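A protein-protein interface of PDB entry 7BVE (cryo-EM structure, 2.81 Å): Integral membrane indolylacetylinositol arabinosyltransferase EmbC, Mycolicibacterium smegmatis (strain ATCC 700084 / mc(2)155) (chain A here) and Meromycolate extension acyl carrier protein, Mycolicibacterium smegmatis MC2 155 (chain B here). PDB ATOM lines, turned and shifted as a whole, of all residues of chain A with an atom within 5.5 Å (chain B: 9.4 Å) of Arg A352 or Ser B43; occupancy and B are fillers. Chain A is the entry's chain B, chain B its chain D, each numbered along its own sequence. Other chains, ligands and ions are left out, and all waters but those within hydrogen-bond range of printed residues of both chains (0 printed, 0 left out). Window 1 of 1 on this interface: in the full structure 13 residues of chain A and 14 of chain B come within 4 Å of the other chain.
The guanidinium group of Arg A352 lies within salt-bridge range of the side-chain carboxylate of Glu B46 (2.7 Å).
The side-chain carboxylate (OE2) of Glu A400 lies within salt-bridge range of the guanidinium group (NH2) of Arg A352 (3.0 Å).
O of Leu A353 is in hydrogen-bond range of N of Ala A547 (3.4 Å).
OG of Ser B43 lies within hydrogen-bond range of OD1 of Asp B40 (3.0 Å).
Among the printed residues, merely in contact across the chains: Gly A354 with Thr B20 (3.3 Å), Ala A547 with Val B19 (3.4 Å), Ala A404 with Val B49 (3.5 Å), Ala A404 with Glu B46 (3.7 Å), Ala A547 with Thr B20 (3.7 Å), Ala A404 with Leu B42 (3.8 Å), Arg A352 with Leu B42 (3.9 Å) and Arg A352 with Ser B43 (3.9997 Å).
Of the printed residues of chain B, Arg A352 touches Leu B42 (3.9 Å), Ser B43 (3.9997 Å) and Glu B46 (2.7 Å).
Printed residues of chain B within 4 Å of Ala A547: Val B19 (3.4 Å) and Thr B20 (3.7 Å).
Pro A550 touches none of the printed residues of chain B.
Printed residues of chain A within 4 Å of Val B19: Ala A547 (3.4 Å).
Printed residues of chain A within 4 Å of Thr B20: Gly A354 and Ala A547.
Leu B37 touches none of the printed residues of chain A.
Of the printed residues of chain A, Leu B42 touches Arg A352 and Ala A404.
Printed residues of chain A within 4 Å of Ser B43: Arg A352 (3.9997 Å).
Of the printed residues of chain A, Glu B46 touches Arg A352 and Ala A404.
The nearest printed residue of chain A that does not touch Ser B43 is Pro A351 (5.8 Å).
Of the 13 printed residues of chain A, 4 touch a printed residue of chain B.
Printed residues of chain A that touch a printed residue of chain B: Arg A352, Gly A354, Ala A404 and Ala A547.
Hydrophobic or aromatic side chains of chain A within 4 Å of the printed part of chain B: Ala A404 and Ala A547.
Of the 26 printed residues of chain B, 6 touch a printed residue of chain A.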
ATOM      1  N   GLU A 348       3.787  13.092 -10.905  1.00  0.00           N
ATOM      2  CA  GLU A 348       3.542  12.077  -9.895  1.00  0.00           C
ATOM      3  C   GLU A 348       3.111  10.750 -10.492  1.00  0.00           C
ATOM      4  O   GLU A 348       3.548   9.700 -10.021  1.00  0.00           O
ATOM      5  CB  GLU A 348       2.498  12.597  -8.896  1.00  0.00           C
ATOM      6  CG  GLU A 348       2.075  11.619  -7.804  1.00  0.00           C
ATOM      7  CD  GLU A 348       3.166  11.244  -6.814  1.00  0.00           C
ATOM      8  OE1 GLU A 348       4.093  12.047  -6.597  1.00  0.00           O
ATOM      9  OE2 GLU A 348       3.088  10.133  -6.246  1.00  0.00           O
ATOM     10  N   VAL A 349       2.298  10.757 -11.543  1.00  0.00           N
ATOM     11  CA  VAL A 349       1.729   9.506 -12.029  1.00  0.00           C
ATOM     12  C   VAL A 349       2.657   8.820 -13.022  1.00  0.00           C
ATOM     13  O   VAL A 349       2.957   7.634 -12.872  1.00  0.00           O
ATOM     14  CB  VAL A 349       0.338   9.745 -12.632  1.00  0.00           C
ATOM     15  CG1 VAL A 349      -0.190   8.468 -13.228  1.00  0.00           C
ATOM     16  CG2 VAL A 349      -0.607  10.259 -11.570  1.00  0.00           C
ATOM     17  N   ILE A 350       3.107   9.529 -14.054  1.00  0.00           N
ATOM     18  CA  ILE A 350       3.923   8.932 -15.120  1.00  0.00           C
ATOM     19  C   ILE A 350       5.282   8.410 -14.636  1.00  0.00           C
ATOM     20  O   ILE A 350       5.630   7.282 -15.012  1.00  0.00           O
ATOM     21  CB  ILE A 350       4.051   9.897 -16.317  1.00  0.00           C
ATOM     22  CG1 ILE A 350       2.732   9.964 -17.080  1.00  0.00           C
ATOM     23  CG2 ILE A 350       5.144   9.501 -17.272  1.00  0.00           C
ATOM     24  CD1 ILE A 350       2.716  10.980 -18.181  1.00  0.00           C
ATOM     25  N   PRO A 351       6.064   9.086 -13.777  1.00  0.00           N
ATOM     26  CA  PRO A 351       7.253   8.411 -13.230  1.00  0.00           C
ATOM     27  C   PRO A 351       6.964   7.309 -12.223  1.00  0.00           C
ATOM     28  O   PRO A 351       7.907   6.642 -11.792  1.00  0.00           O
ATOM     29  CB  PRO A 351       8.040   9.550 -12.577  1.00  0.00           C
ATOM     30  CG  PRO A 351       7.091  10.567 -12.324  1.00  0.00           C
ATOM     31  CD  PRO A 351       6.124  10.520 -13.440  1.00  0.00           C
ATOM     32  N   ARG A 352       5.713   7.094 -11.834  1.00  0.00           N
ATOM     33  CA  ARG A 352       5.358   5.992 -10.954  1.00  0.00           C
ATOM     34  C   ARG A 352       5.043   4.721 -11.725  1.00  0.00           C
ATOM     35  O   ARG A 352       5.334   3.622 -11.244  1.00  0.00           O
ATOM     36  CB  ARG A 352       4.162   6.397 -10.087  1.00  0.00           C
ATOM     37  CG  ARG A 352       3.696   5.375  -9.094  1.00  0.00           C
ATOM     38  CD  ARG A 352       4.746   5.134  -8.046  1.00  0.00           C
ATOM     39  NE  ARG A 352       4.313   4.123  -7.093  1.00  0.00           N
ATOM     40  CZ  ARG A 352       5.121   3.533  -6.224  1.00  0.00           C
ATOM     41  NH1 ARG A 352       6.406   3.853  -6.195  1.00  0.00           N
ATOM     42  NH2 ARG A 352       4.648   2.617  -5.394  1.00  0.00           N
ATOM     43  N   LEU A 353       4.512   4.841 -12.931  1.00  0.00           N
ATOM     44  CA  LEU A 353       4.107   3.704 -13.749  1.00  0.00           C
ATOM     45  C   LEU A 353       5.254   2.937 -14.338  1.00  0.00           C
ATOM     46  O   LEU A 353       4.954   2.125 -15.196  1.00  0.00           O
ATOM     47  CB  LEU A 353       3.195   4.157 -14.885  1.00  0.00           C
ATOM     48  CG  LEU A 353       1.813   4.698 -14.550  1.00  0.00           C
ATOM     49  CD1 LEU A 353       1.148   5.187 -15.810  1.00  0.00           C
ATOM     50  CD2 LEU A 353       0.977   3.640 -13.893  1.00  0.00           C
ATOM     51  N   GLY A 354       6.527   3.101 -14.026  1.00  0.00           N
ATOM     52  CA  GLY A 354       7.534   2.214 -14.552  1.00  0.00           C
ATOM     53  C   GLY A 354       8.667   2.981 -15.163  1.00  0.00           C
ATOM     54  O   GLY A 354       8.755   4.203 -15.048  1.00  0.00           O
ATOM     55  N   TRP A 396      -5.977   8.708  -5.529  1.00  0.00           N
ATOM     56  CA  TRP A 396      -5.103   7.626  -5.987  1.00  0.00           C
ATOM     57  C   TRP A 396      -3.645   7.883  -5.628  1.00  0.00           C
ATOM     58  O   TRP A 396      -2.919   6.952  -5.269  1.00  0.00           O
ATOM     59  CB  TRP A 396      -5.231   7.435  -7.493  1.00  0.00           C
ATOM     60  CG  TRP A 396      -4.423   6.280  -8.015  1.00  0.00           C
ATOM     61  CD1 TRP A 396      -4.689   4.962  -7.857  1.00  0.00           C
ATOM     62  CD2 TRP A 396      -3.183   6.347  -8.724  1.00  0.00           C
ATOM     63  NE1 TRP A 396      -3.727   4.199  -8.455  1.00  0.00           N
ATOM     64  CE2 TRP A 396      -2.782   5.027  -8.989  1.00  0.00           C
ATOM     65  CE3 TRP A 396      -2.376   7.396  -9.164  1.00  0.00           C
ATOM     66  CZ2 TRP A 396      -1.620   4.729  -9.679  1.00  0.00           C
ATOM     67  CZ3 TRP A 396      -1.218   7.096  -9.834  1.00  0.00           C
ATOM     68  CH2 TRP A 396      -0.847   5.775 -10.087  1.00  0.00           C
ATOM     69  N   GLU A 400      -1.402   5.513  -3.189  1.00  0.00           N
ATOM     70  CA  GLU A 400      -0.182   4.920  -3.726  1.00  0.00           C
ATOM     71  C   GLU A 400       1.034   5.265  -2.874  1.00  0.00           C
ATOM     72  O   GLU A 400       1.921   4.426  -2.666  1.00  0.00           O
ATOM     73  CB  GLU A 400       0.013   5.401  -5.157  1.00  0.00           C
ATOM     74  CG  GLU A 400       1.140   4.740  -5.880  1.00  0.00           C
ATOM     75  CD  GLU A 400       0.834   3.303  -6.222  1.00  0.00           C
ATOM     76  OE1 GLU A 400      -0.352   2.976  -6.433  1.00  0.00           O
ATOM     77  OE2 GLU A 400       1.784   2.498  -6.266  1.00  0.00           O
ATOM     78  N   ALA A 404       3.496   2.621  -0.849  1.00  0.00           N
ATOM     79  CA  ALA A 404       4.941   2.596  -1.059  1.00  0.00           C
ATOM     80  C   ALA A 404       5.711   2.715   0.253  1.00  0.00           C
ATOM     81  O   ALA A 404       6.530   1.854   0.583  1.00  0.00           O
ATOM     82  CB  ALA A 404       5.335   3.717  -2.015  1.00  0.00           C
ATOM     83  N   ALA A 547       5.420  -1.015 -13.846  1.00  0.00           N
ATOM     84  CA  ALA A 547       5.179  -1.591 -12.538  1.00  0.00           C
ATOM     85  C   ALA A 547       3.824  -2.285 -12.512  1.00  0.00           C
ATOM     86  O   ALA A 547       2.894  -1.927 -13.237  1.00  0.00           O
ATOM     87  CB  ALA A 547       5.242  -0.516 -11.458  1.00  0.00           C
ATOM     88  N   PRO A 550       0.567  -0.356  -9.607  1.00  0.00           N
ATOM     89  CA  PRO A 550      -0.073   0.858 -10.146  1.00  0.00           C
ATOM     90  C   PRO A 550      -0.827   0.666 -11.448  1.00  0.00           C
ATOM     91  O   PRO A 550      -1.872   1.298 -11.632  1.00  0.00           O
ATOM     92  CB  PRO A 550       1.114   1.806 -10.328  1.00  0.00           C
ATOM     93  CG  PRO A 550       2.062   1.389  -9.326  1.00  0.00           C
ATOM     94  CD  PRO A 550       1.958  -0.076  -9.208  1.00  0.00           C
ATOM     95  N   ARG A 553      -4.078  -0.999 -10.577  1.00  0.00           N
ATOM     96  CA  ARG A 553      -4.985  -0.125  -9.846  1.00  0.00           C
ATOM     97  C   ARG A 553      -5.574   0.974 -10.725  1.00  0.00           C
ATOM     98  O   ARG A 553      -6.730   1.357 -10.519  1.00  0.00           O
ATOM     99  CB  ARG A 553      -4.271   0.448  -8.625  1.00  0.00           C
ATOM    100  CG  ARG A 553      -4.097  -0.589  -7.517  1.00  0.00           C
ATOM    101  CD  ARG A 553      -3.725   0.017  -6.175  1.00  0.00           C
ATOM    102  NE  ARG A 553      -2.346   0.474  -6.080  1.00  0.00           N
ATOM    103  CZ  ARG A 553      -1.355  -0.272  -5.610  1.00  0.00           C
ATOM    104  NH1 ARG A 553      -1.597  -1.504  -5.191  1.00  0.00           N
ATOM    105  NH2 ARG A 553      -0.124   0.214  -5.546  1.00  0.00           N
ATOM    106  N   LEU B  12      16.802 -10.040  -5.309  1.00  0.00           N
ATOM    107  CA  LEU B  12      16.775  -8.584  -5.305  1.00  0.00           C
ATOM    108  C   LEU B  12      16.445  -8.041  -6.692  1.00  0.00           C
ATOM    109  O   LEU B  12      15.790  -7.000  -6.818  1.00  0.00           O
ATOM    110  CB  LEU B  12      18.108  -8.044  -4.797  1.00  0.00           C
ATOM    111  CG  LEU B  12      18.165  -6.550  -4.508  1.00  0.00           C
ATOM    112  CD1 LEU B  12      17.116  -6.202  -3.476  1.00  0.00           C
ATOM    113  CD2 LEU B  12      19.533  -6.183  -3.993  1.00  0.00           C
ATOM    114  N   ILE B  15      12.675  -8.254  -6.854  1.00  0.00           N
ATOM    115  CA  ILE B  15      12.037  -7.158  -6.121  1.00  0.00           C
ATOM    116  C   ILE B  15      12.131  -5.849  -6.903  1.00  0.00           C
ATOM    117  O   ILE B  15      11.153  -5.094  -6.995  1.00  0.00           O
ATOM    118  CB  ILE B  15      12.651  -7.029  -4.715  1.00  0.00           C
ATOM    119  CG1 ILE B  15      12.319  -8.257  -3.872  1.00  0.00           C
ATOM    120  CG2 ILE B  15      12.166  -5.786  -4.007  1.00  0.00           C
ATOM    121  CD1 ILE B  15      13.041  -8.284  -2.552  1.00  0.00           C
ATOM    122  N   ILE B  16      13.294  -5.576  -7.507  1.00  0.00           N
ATOM    123  CA  ILE B  16      13.467  -4.365  -8.309  1.00  0.00           C
ATOM    124  C   ILE B  16      12.597  -4.411  -9.563  1.00  0.00           C
ATOM    125  O   ILE B  16      12.009  -3.395  -9.957  1.00  0.00           O
ATOM    126  CB  ILE B  16      14.961  -4.162  -8.631  1.00  0.00           C
ATOM    127  CG1 ILE B  16      15.718  -3.783  -7.360  1.00  0.00           C
ATOM    128  CG2 ILE B  16      15.191  -3.103  -9.693  1.00  0.00           C
ATOM    129  CD1 ILE B  16      17.206  -3.789  -7.517  1.00  0.00           C
ATOM    130  N   GLU B  18       9.687  -6.019  -9.825  1.00  0.00           N
ATOM    131  CA  GLU B  18       8.300  -5.840  -9.411  1.00  0.00           C
ATOM    132  C   GLU B  18       7.996  -4.389  -9.064  1.00  0.00           C
ATOM    133  O   GLU B  18       6.973  -3.846  -9.496  1.00  0.00           O
ATOM    134  CB  GLU B  18       7.990  -6.739  -8.219  1.00  0.00           C
ATOM    135  CG  GLU B  18       6.571  -6.613  -7.732  1.00  0.00           C
ATOM    136  CD  GLU B  18       6.286  -7.484  -6.537  1.00  0.00           C
ATOM    137  OE1 GLU B  18       7.202  -8.208  -6.095  1.00  0.00           O
ATOM    138  OE2 GLU B  18       5.147  -7.433  -6.027  1.00  0.00           O
ATOM    139  N   VAL B  19       8.877  -3.742  -8.298  1.00  0.00           N
ATOM    140  CA  VAL B  19       8.614  -2.379  -7.841  1.00  0.00           C
ATOM    141  C   VAL B  19       8.739  -1.386  -8.988  1.00  0.00           C
ATOM    142  O   VAL B  19       7.838  -0.576  -9.225  1.00  0.00           O
ATOM    143  CB  VAL B  19       9.547  -2.019  -6.677  1.00  0.00           C
ATOM    144  CG1 VAL B  19       9.443  -0.557  -6.355  1.00  0.00           C
ATOM    145  CG2 VAL B  19       9.187  -2.836  -5.461  1.00  0.00           C
ATOM    146  N   THR B  20       9.845  -1.434  -9.730  1.00  0.00           N
ATOM    147  CA  THR B  20      10.103  -0.414 -10.737  1.00  0.00           C
ATOM    148  C   THR B  20       9.738  -0.876 -12.143  1.00  0.00           C
ATOM    149  O   THR B  20       8.912  -0.249 -12.807  1.00  0.00           O
ATOM    150  CB  THR B  20      11.568   0.013 -10.690  1.00  0.00           C
ATOM    151  OG1 THR B  20      11.936   0.274  -9.335  1.00  0.00           O
ATOM    152  CG2 THR B  20      11.726   1.302 -11.465  1.00  0.00           C
ATOM    153  N   GLY B  21      10.335  -1.958 -12.615  1.00  0.00           N
ATOM    154  CA  GLY B  21      10.029  -2.420 -13.951  1.00  0.00           C
ATOM    155  C   GLY B  21      11.239  -2.707 -14.814  1.00  0.00           C
ATOM    156  O   GLY B  21      11.095  -2.968 -16.008  1.00  0.00           O
ATOM    157  N   ILE B  22      12.437  -2.655 -14.233  1.00  0.00           N
ATOM    158  CA  ILE B  22      13.637  -3.040 -14.964  1.00  0.00           C
ATOM    159  C   ILE B  22      13.649  -4.554 -15.123  1.00  0.00           C
ATOM    160  O   ILE B  22      13.345  -5.290 -14.177  1.00  0.00           O
ATOM    161  CB  ILE B  22      14.901  -2.539 -14.243  1.00  0.00           C
ATOM    162  CG1 ILE B  22      14.948  -1.018 -14.168  1.00  0.00           C
ATOM    163  CG2 ILE B  22      16.163  -2.994 -14.934  1.00  0.00           C
ATOM    164  CD1 ILE B  22      14.607  -0.474 -12.836  1.00  0.00           C
ATOM    165  N   PHE B  33      22.512   2.785  -8.478  1.00  0.00           N
ATOM    166  CA  PHE B  33      21.067   2.952  -8.381  1.00  0.00           C
ATOM    167  C   PHE B  33      20.577   4.200  -9.106  1.00  0.00           C
ATOM    168  O   PHE B  33      19.793   4.111 -10.056  1.00  0.00           O
ATOM    169  CB  PHE B  33      20.649   2.996  -6.915  1.00  0.00           C
ATOM    170  CG  PHE B  33      20.475   1.648  -6.286  1.00  0.00           C
ATOM    171  CD1 PHE B  33      20.311   0.517  -7.068  1.00  0.00           C
ATOM    172  CD2 PHE B  33      20.455   1.513  -4.908  1.00  0.00           C
ATOM    173  CE1 PHE B  33      20.138  -0.723  -6.489  1.00  0.00           C
ATOM    174  CE2 PHE B  33      20.287   0.277  -4.325  1.00  0.00           C
ATOM    175  CZ  PHE B  33      20.128  -0.843  -5.117  1.00  0.00           C
ATOM    176  N   VAL B  34      21.029   5.374  -8.672  1.00  0.00           N
ATOM    177  CA  VAL B  34      20.476   6.634  -9.158  1.00  0.00           C
ATOM    178  C   VAL B  34      21.255   7.152 -10.359  1.00  0.00           C
ATOM    179  O   VAL B  34      21.090   8.305 -10.768  1.00  0.00           O
ATOM    180  CB  VAL B  34      20.454   7.687  -8.037  1.00  0.00           C
ATOM    181  CG1 VAL B  34      19.550   7.236  -6.910  1.00  0.00           C
ATOM    182  CG2 VAL B  34      21.859   7.931  -7.524  1.00  0.00           C
ATOM    183  N   LEU B  37      20.502   2.717 -13.284  1.00  0.00           N
ATOM    184  CA  LEU B  37      19.135   2.235 -13.150  1.00  0.00           C
ATOM    185  C   LEU B  37      18.133   3.377 -13.049  1.00  0.00           C
ATOM    186  O   LEU B  37      16.985   3.212 -13.477  1.00  0.00           O
ATOM    187  CB  LEU B  37      19.019   1.315 -11.934  1.00  0.00           C
ATOM    188  CG  LEU B  37      19.766  -0.015 -12.043  1.00  0.00           C
ATOM    189  CD1 LEU B  37      19.664  -0.804 -10.755  1.00  0.00           C
ATOM    190  CD2 LEU B  37      19.235  -0.825 -13.204  1.00  0.00           C
ATOM    191  N   ASP B  38      18.559   4.522 -12.497  1.00  0.00           N
ATOM    192  CA  ASP B  38      17.777   5.762 -12.387  1.00  0.00           C
ATOM    193  C   ASP B  38      16.486   5.532 -11.596  1.00  0.00           C
ATOM    194  O   ASP B  38      15.373   5.675 -12.101  1.00  0.00           O
ATOM    195  CB  ASP B  38      17.493   6.361 -13.771  1.00  0.00           C
ATOM    196  CG  ASP B  38      17.017   7.805 -13.711  1.00  0.00           C
ATOM    197  OD1 ASP B  38      16.921   8.379 -12.606  1.00  0.00           O
ATOM    198  OD2 ASP B  38      16.732   8.369 -14.788  1.00  0.00           O
ATOM    199  N   ILE B  39      16.661   5.172 -10.329  1.00  0.00           N
ATOM    200  CA  ILE B  39      15.561   4.823  -9.440  1.00  0.00           C
ATOM    201  C   ILE B  39      15.363   5.959  -8.446  1.00  0.00           C
ATOM    202  O   ILE B  39      16.312   6.376  -7.773  1.00  0.00           O
ATOM    203  CB  ILE B  39      15.830   3.484  -8.731  1.00  0.00           C
ATOM    204  CG1 ILE B  39      15.820   2.343  -9.746  1.00  0.00           C
ATOM    205  CG2 ILE B  39      14.812   3.219  -7.669  1.00  0.00           C
ATOM    206  CD1 ILE B  39      16.271   1.028  -9.186  1.00  0.00           C
ATOM    207  N   ASP B  40      14.133   6.463  -8.363  1.00  0.00           N
ATOM    208  CA  ASP B  40      13.799   7.593  -7.505  1.00  0.00           C
ATOM    209  C   ASP B  40      13.645   7.130  -6.058  1.00  0.00           C
ATOM    210  O   ASP B  40      13.742   5.940  -5.751  1.00  0.00           O
ATOM    211  CB  ASP B  40      12.555   8.298  -8.037  1.00  0.00           C
ATOM    212  CG  ASP B  40      11.395   7.347  -8.272  1.00  0.00           C
ATOM    213  OD1 ASP B  40      11.585   6.123  -8.132  1.00  0.00           O
ATOM    214  OD2 ASP B  40      10.289   7.824  -8.601  1.00  0.00           O
ATOM    215  N   SER B  41      13.376   8.070  -5.150  1.00  0.00           N
ATOM    216  CA  SER B  41      13.481   7.784  -3.722  1.00  0.00           C
ATOM    217  C   SER B  41      12.251   7.072  -3.175  1.00  0.00           C
ATOM    218  O   SER B  41      12.354   6.328  -2.188  1.00  0.00           O
ATOM    219  CB  SER B  41      13.721   9.077  -2.949  1.00  0.00           C
ATOM    220  OG  SER B  41      12.595   9.930  -3.030  1.00  0.00           O
ATOM    221  N   LEU B  42      11.083   7.297  -3.782  1.00  0.00           N
ATOM    222  CA  LEU B  42       9.887   6.581  -3.353  1.00  0.00           C
ATOM    223  C   LEU B  42      10.015   5.096  -3.666  1.00  0.00           C
ATOM    224  O   LEU B  42       9.620   4.241  -2.861  1.00  0.00           O
ATOM    225  CB  LEU B  42       8.650   7.182  -4.018  1.00  0.00           C
ATOM    226  CG  LEU B  42       7.293   6.682  -3.522  1.00  0.00           C
ATOM    227  CD1 LEU B  42       7.109   7.054  -2.073  1.00  0.00           C
ATOM    228  CD2 LEU B  42       6.160   7.244  -4.355  1.00  0.00           C
ATOM    229  N   SER B  43      10.637   4.772  -4.802  1.00  0.00           N
ATOM    230  CA  SER B  43      10.938   3.380  -5.106  1.00  0.00           C
ATOM    231  C   SER B  43      12.052   2.833  -4.223  1.00  0.00           C
ATOM    232  O   SER B  43      12.081   1.627  -3.977  1.00  0.00           O
ATOM    233  CB  SER B  43      11.302   3.228  -6.576  1.00  0.00           C
ATOM    234  OG  SER B  43      10.205   3.543  -7.407  1.00  0.00           O
ATOM    235  N   MET B  44      12.957   3.684  -3.725  1.00  0.00           N
ATOM    236  CA  MET B  44      13.947   3.227  -2.750  1.00  0.00           C
ATOM    237  C   MET B  44      13.281   2.778  -1.464  1.00  0.00           C
ATOM    238  O   MET B  44      13.613   1.722  -0.909  1.00  0.00           O
ATOM    239  CB  MET B  44      14.945   4.331  -2.423  1.00  0.00           C
ATOM    240  CG  MET B  44      15.825   4.749  -3.542  1.00  0.00           C
ATOM    241  SD  MET B  44      16.898   3.443  -4.105  1.00  0.00           S
ATOM    242  CE  MET B  44      17.603   4.314  -5.481  1.00  0.00           C
ATOM    243  N   VAL B  45      12.328   3.576  -0.974  1.00  0.00           N
ATOM    244  CA  VAL B  45      11.610   3.217   0.247  1.00  0.00           C
ATOM    245  C   VAL B  45      10.746   1.979   0.014  1.00  0.00           C
ATOM    246  O   VAL B  45      10.617   1.118   0.894  1.00  0.00           O
ATOM    247  CB  VAL B  45      10.789   4.421   0.744  1.00  0.00           C
ATOM    248  CG1 VAL B  45      10.037   4.090   2.013  1.00  0.00           C
ATOM    249  CG2 VAL B  45      11.697   5.603   0.971  1.00  0.00           C
ATOM    250  N   GLU B  46      10.205   1.834  -1.199  1.00  0.00           N
ATOM    251  CA  GLU B  46       9.378   0.669  -1.498  1.00  0.00           C
ATOM    252  C   GLU B  46      10.211  -0.607  -1.603  1.00  0.00           C
ATOM    253  O   GLU B  46       9.788  -1.668  -1.132  1.00  0.00           O
ATOM    254  CB  GLU B  46       8.588   0.911  -2.779  1.00  0.00           C
ATOM    255  CG  GLU B  46       7.530  -0.128  -3.056  1.00  0.00           C
ATOM    256  CD  GLU B  46       6.652   0.246  -4.229  1.00  0.00           C
ATOM    257  OE1 GLU B  46       6.923   1.285  -4.865  1.00  0.00           O
ATOM    258  OE2 GLU B  46       5.677  -0.486  -4.505  1.00  0.00           O
ATOM    259  N   ILE B  47      11.406  -0.524  -2.193  1.00  0.00           N
ATOM    260  CA  ILE B  47      12.315  -1.670  -2.226  1.00  0.00           C
ATOM    261  C   ILE B  47      12.777  -2.022  -0.816  1.00  0.00           C
ATOM    262  O   ILE B  47      12.887  -3.205  -0.460  1.00  0.00           O
ATOM    263  CB  ILE B  47      13.492  -1.378  -3.181  1.00  0.00           C
ATOM    264  CG1 ILE B  47      13.012  -1.379  -4.630  1.00  0.00           C
ATOM    265  CG2 ILE B  47      14.607  -2.386  -3.042  1.00  0.00           C
ATOM    266  CD1 ILE B  47      14.012  -0.819  -5.603  1.00  0.00           C
ATOM    267  N   ALA B  48      12.988  -1.006   0.026  1.00  0.00           N
ATOM    268  CA  ALA B  48      13.400  -1.245   1.405  1.00  0.00           C
ATOM    269  C   ALA B  48      12.316  -1.964   2.202  1.00  0.00           C
ATOM    270  O   ALA B  48      12.606  -2.897   2.960  1.00  0.00           O
ATOM    271  CB  ALA B  48      13.773   0.076   2.072  1.00  0.00           C
ATOM    272  N   VAL B  49      11.050  -1.578   2.015  1.00  0.00           N
ATOM    273  CA  VAL B  49      10.000  -2.256   2.769  1.00  0.00           C
ATOM    274  C   VAL B  49       9.678  -3.630   2.186  1.00  0.00           C
ATOM    275  O   VAL B  49       9.294  -4.532   2.942  1.00  0.00           O
ATOM    276  CB  VAL B  49       8.728  -1.389   2.899  1.00  0.00           C
ATOM    277  CG1 VAL B  49       9.053  -0.081   3.587  1.00  0.00           C
ATOM    278  CG2 VAL B  49       8.055  -1.141   1.576  1.00  0.00           C
ATOM    279  N   GLN B  50       9.881  -3.847   0.880  1.00  0.00           N
ATOM    280  CA  GLN B  50       9.749  -5.200   0.340  1.00  0.00           C
ATOM    281  C   GLN B  50      10.830  -6.134   0.875  1.00  0.00           C
ATOM    282  O   GLN B  50      10.549  -7.297   1.196  1.00  0.00           O
ATOM    283  CB  GLN B  50       9.799  -5.175  -1.188  1.00  0.00           C
ATOM    284  CG  GLN B  50       8.595  -4.566  -1.865  1.00  0.00           C
ATOM    285  CD  GLN B  50       7.359  -5.391  -1.673  1.00  0.00           C
ATOM    286  OE1 GLN B  50       7.413  -6.619  -1.678  1.00  0.00           O
ATOM    287  NE2 GLN B  50       6.226  -4.725  -1.504  1.00  0.00           N
ATOM    288  N   THR B  51      12.065  -5.639   0.984  1.00  0.00           N
ATOM    289  CA  THR B  51      13.150  -6.463   1.506  1.00  0.00           C
ATOM    290  C   THR B  51      12.982  -6.700   3.004  1.00  0.00           C
ATOM    291  O   THR B  51      13.325  -7.775   3.513  1.00  0.00           O
ATOM    292  CB  THR B  51      14.491  -5.801   1.188  1.00  0.00           C
ATOM    293  OG1 THR B  51      14.563  -5.547  -0.219  1.00  0.00           O
ATOM    294  CG2 THR B  51      15.649  -6.701   1.546  1.00  0.00           C
ATOM    295  N   LEU B  64      20.292   4.468   4.572  1.00  0.00           N
ATOM    296  CA  LEU B  64      19.475   5.389   3.794  1.00  0.00           C
ATOM    297  C   LEU B  64      20.333   6.410   3.061  1.00  0.00           C
ATOM    298  O   LEU B  64      19.943   6.880   1.987  1.00  0.00           O
ATOM    299  CB  LEU B  64      18.468   6.093   4.711  1.00  0.00           C
ATOM    300  CG  LEU B  64      17.366   6.946   4.072  1.00  0.00           C
ATOM    301  CD1 LEU B  64      16.425   6.072   3.254  1.00  0.00           C
ATOM    302  CD2 LEU B  64      16.593   7.734   5.118  1.00  0.00           C
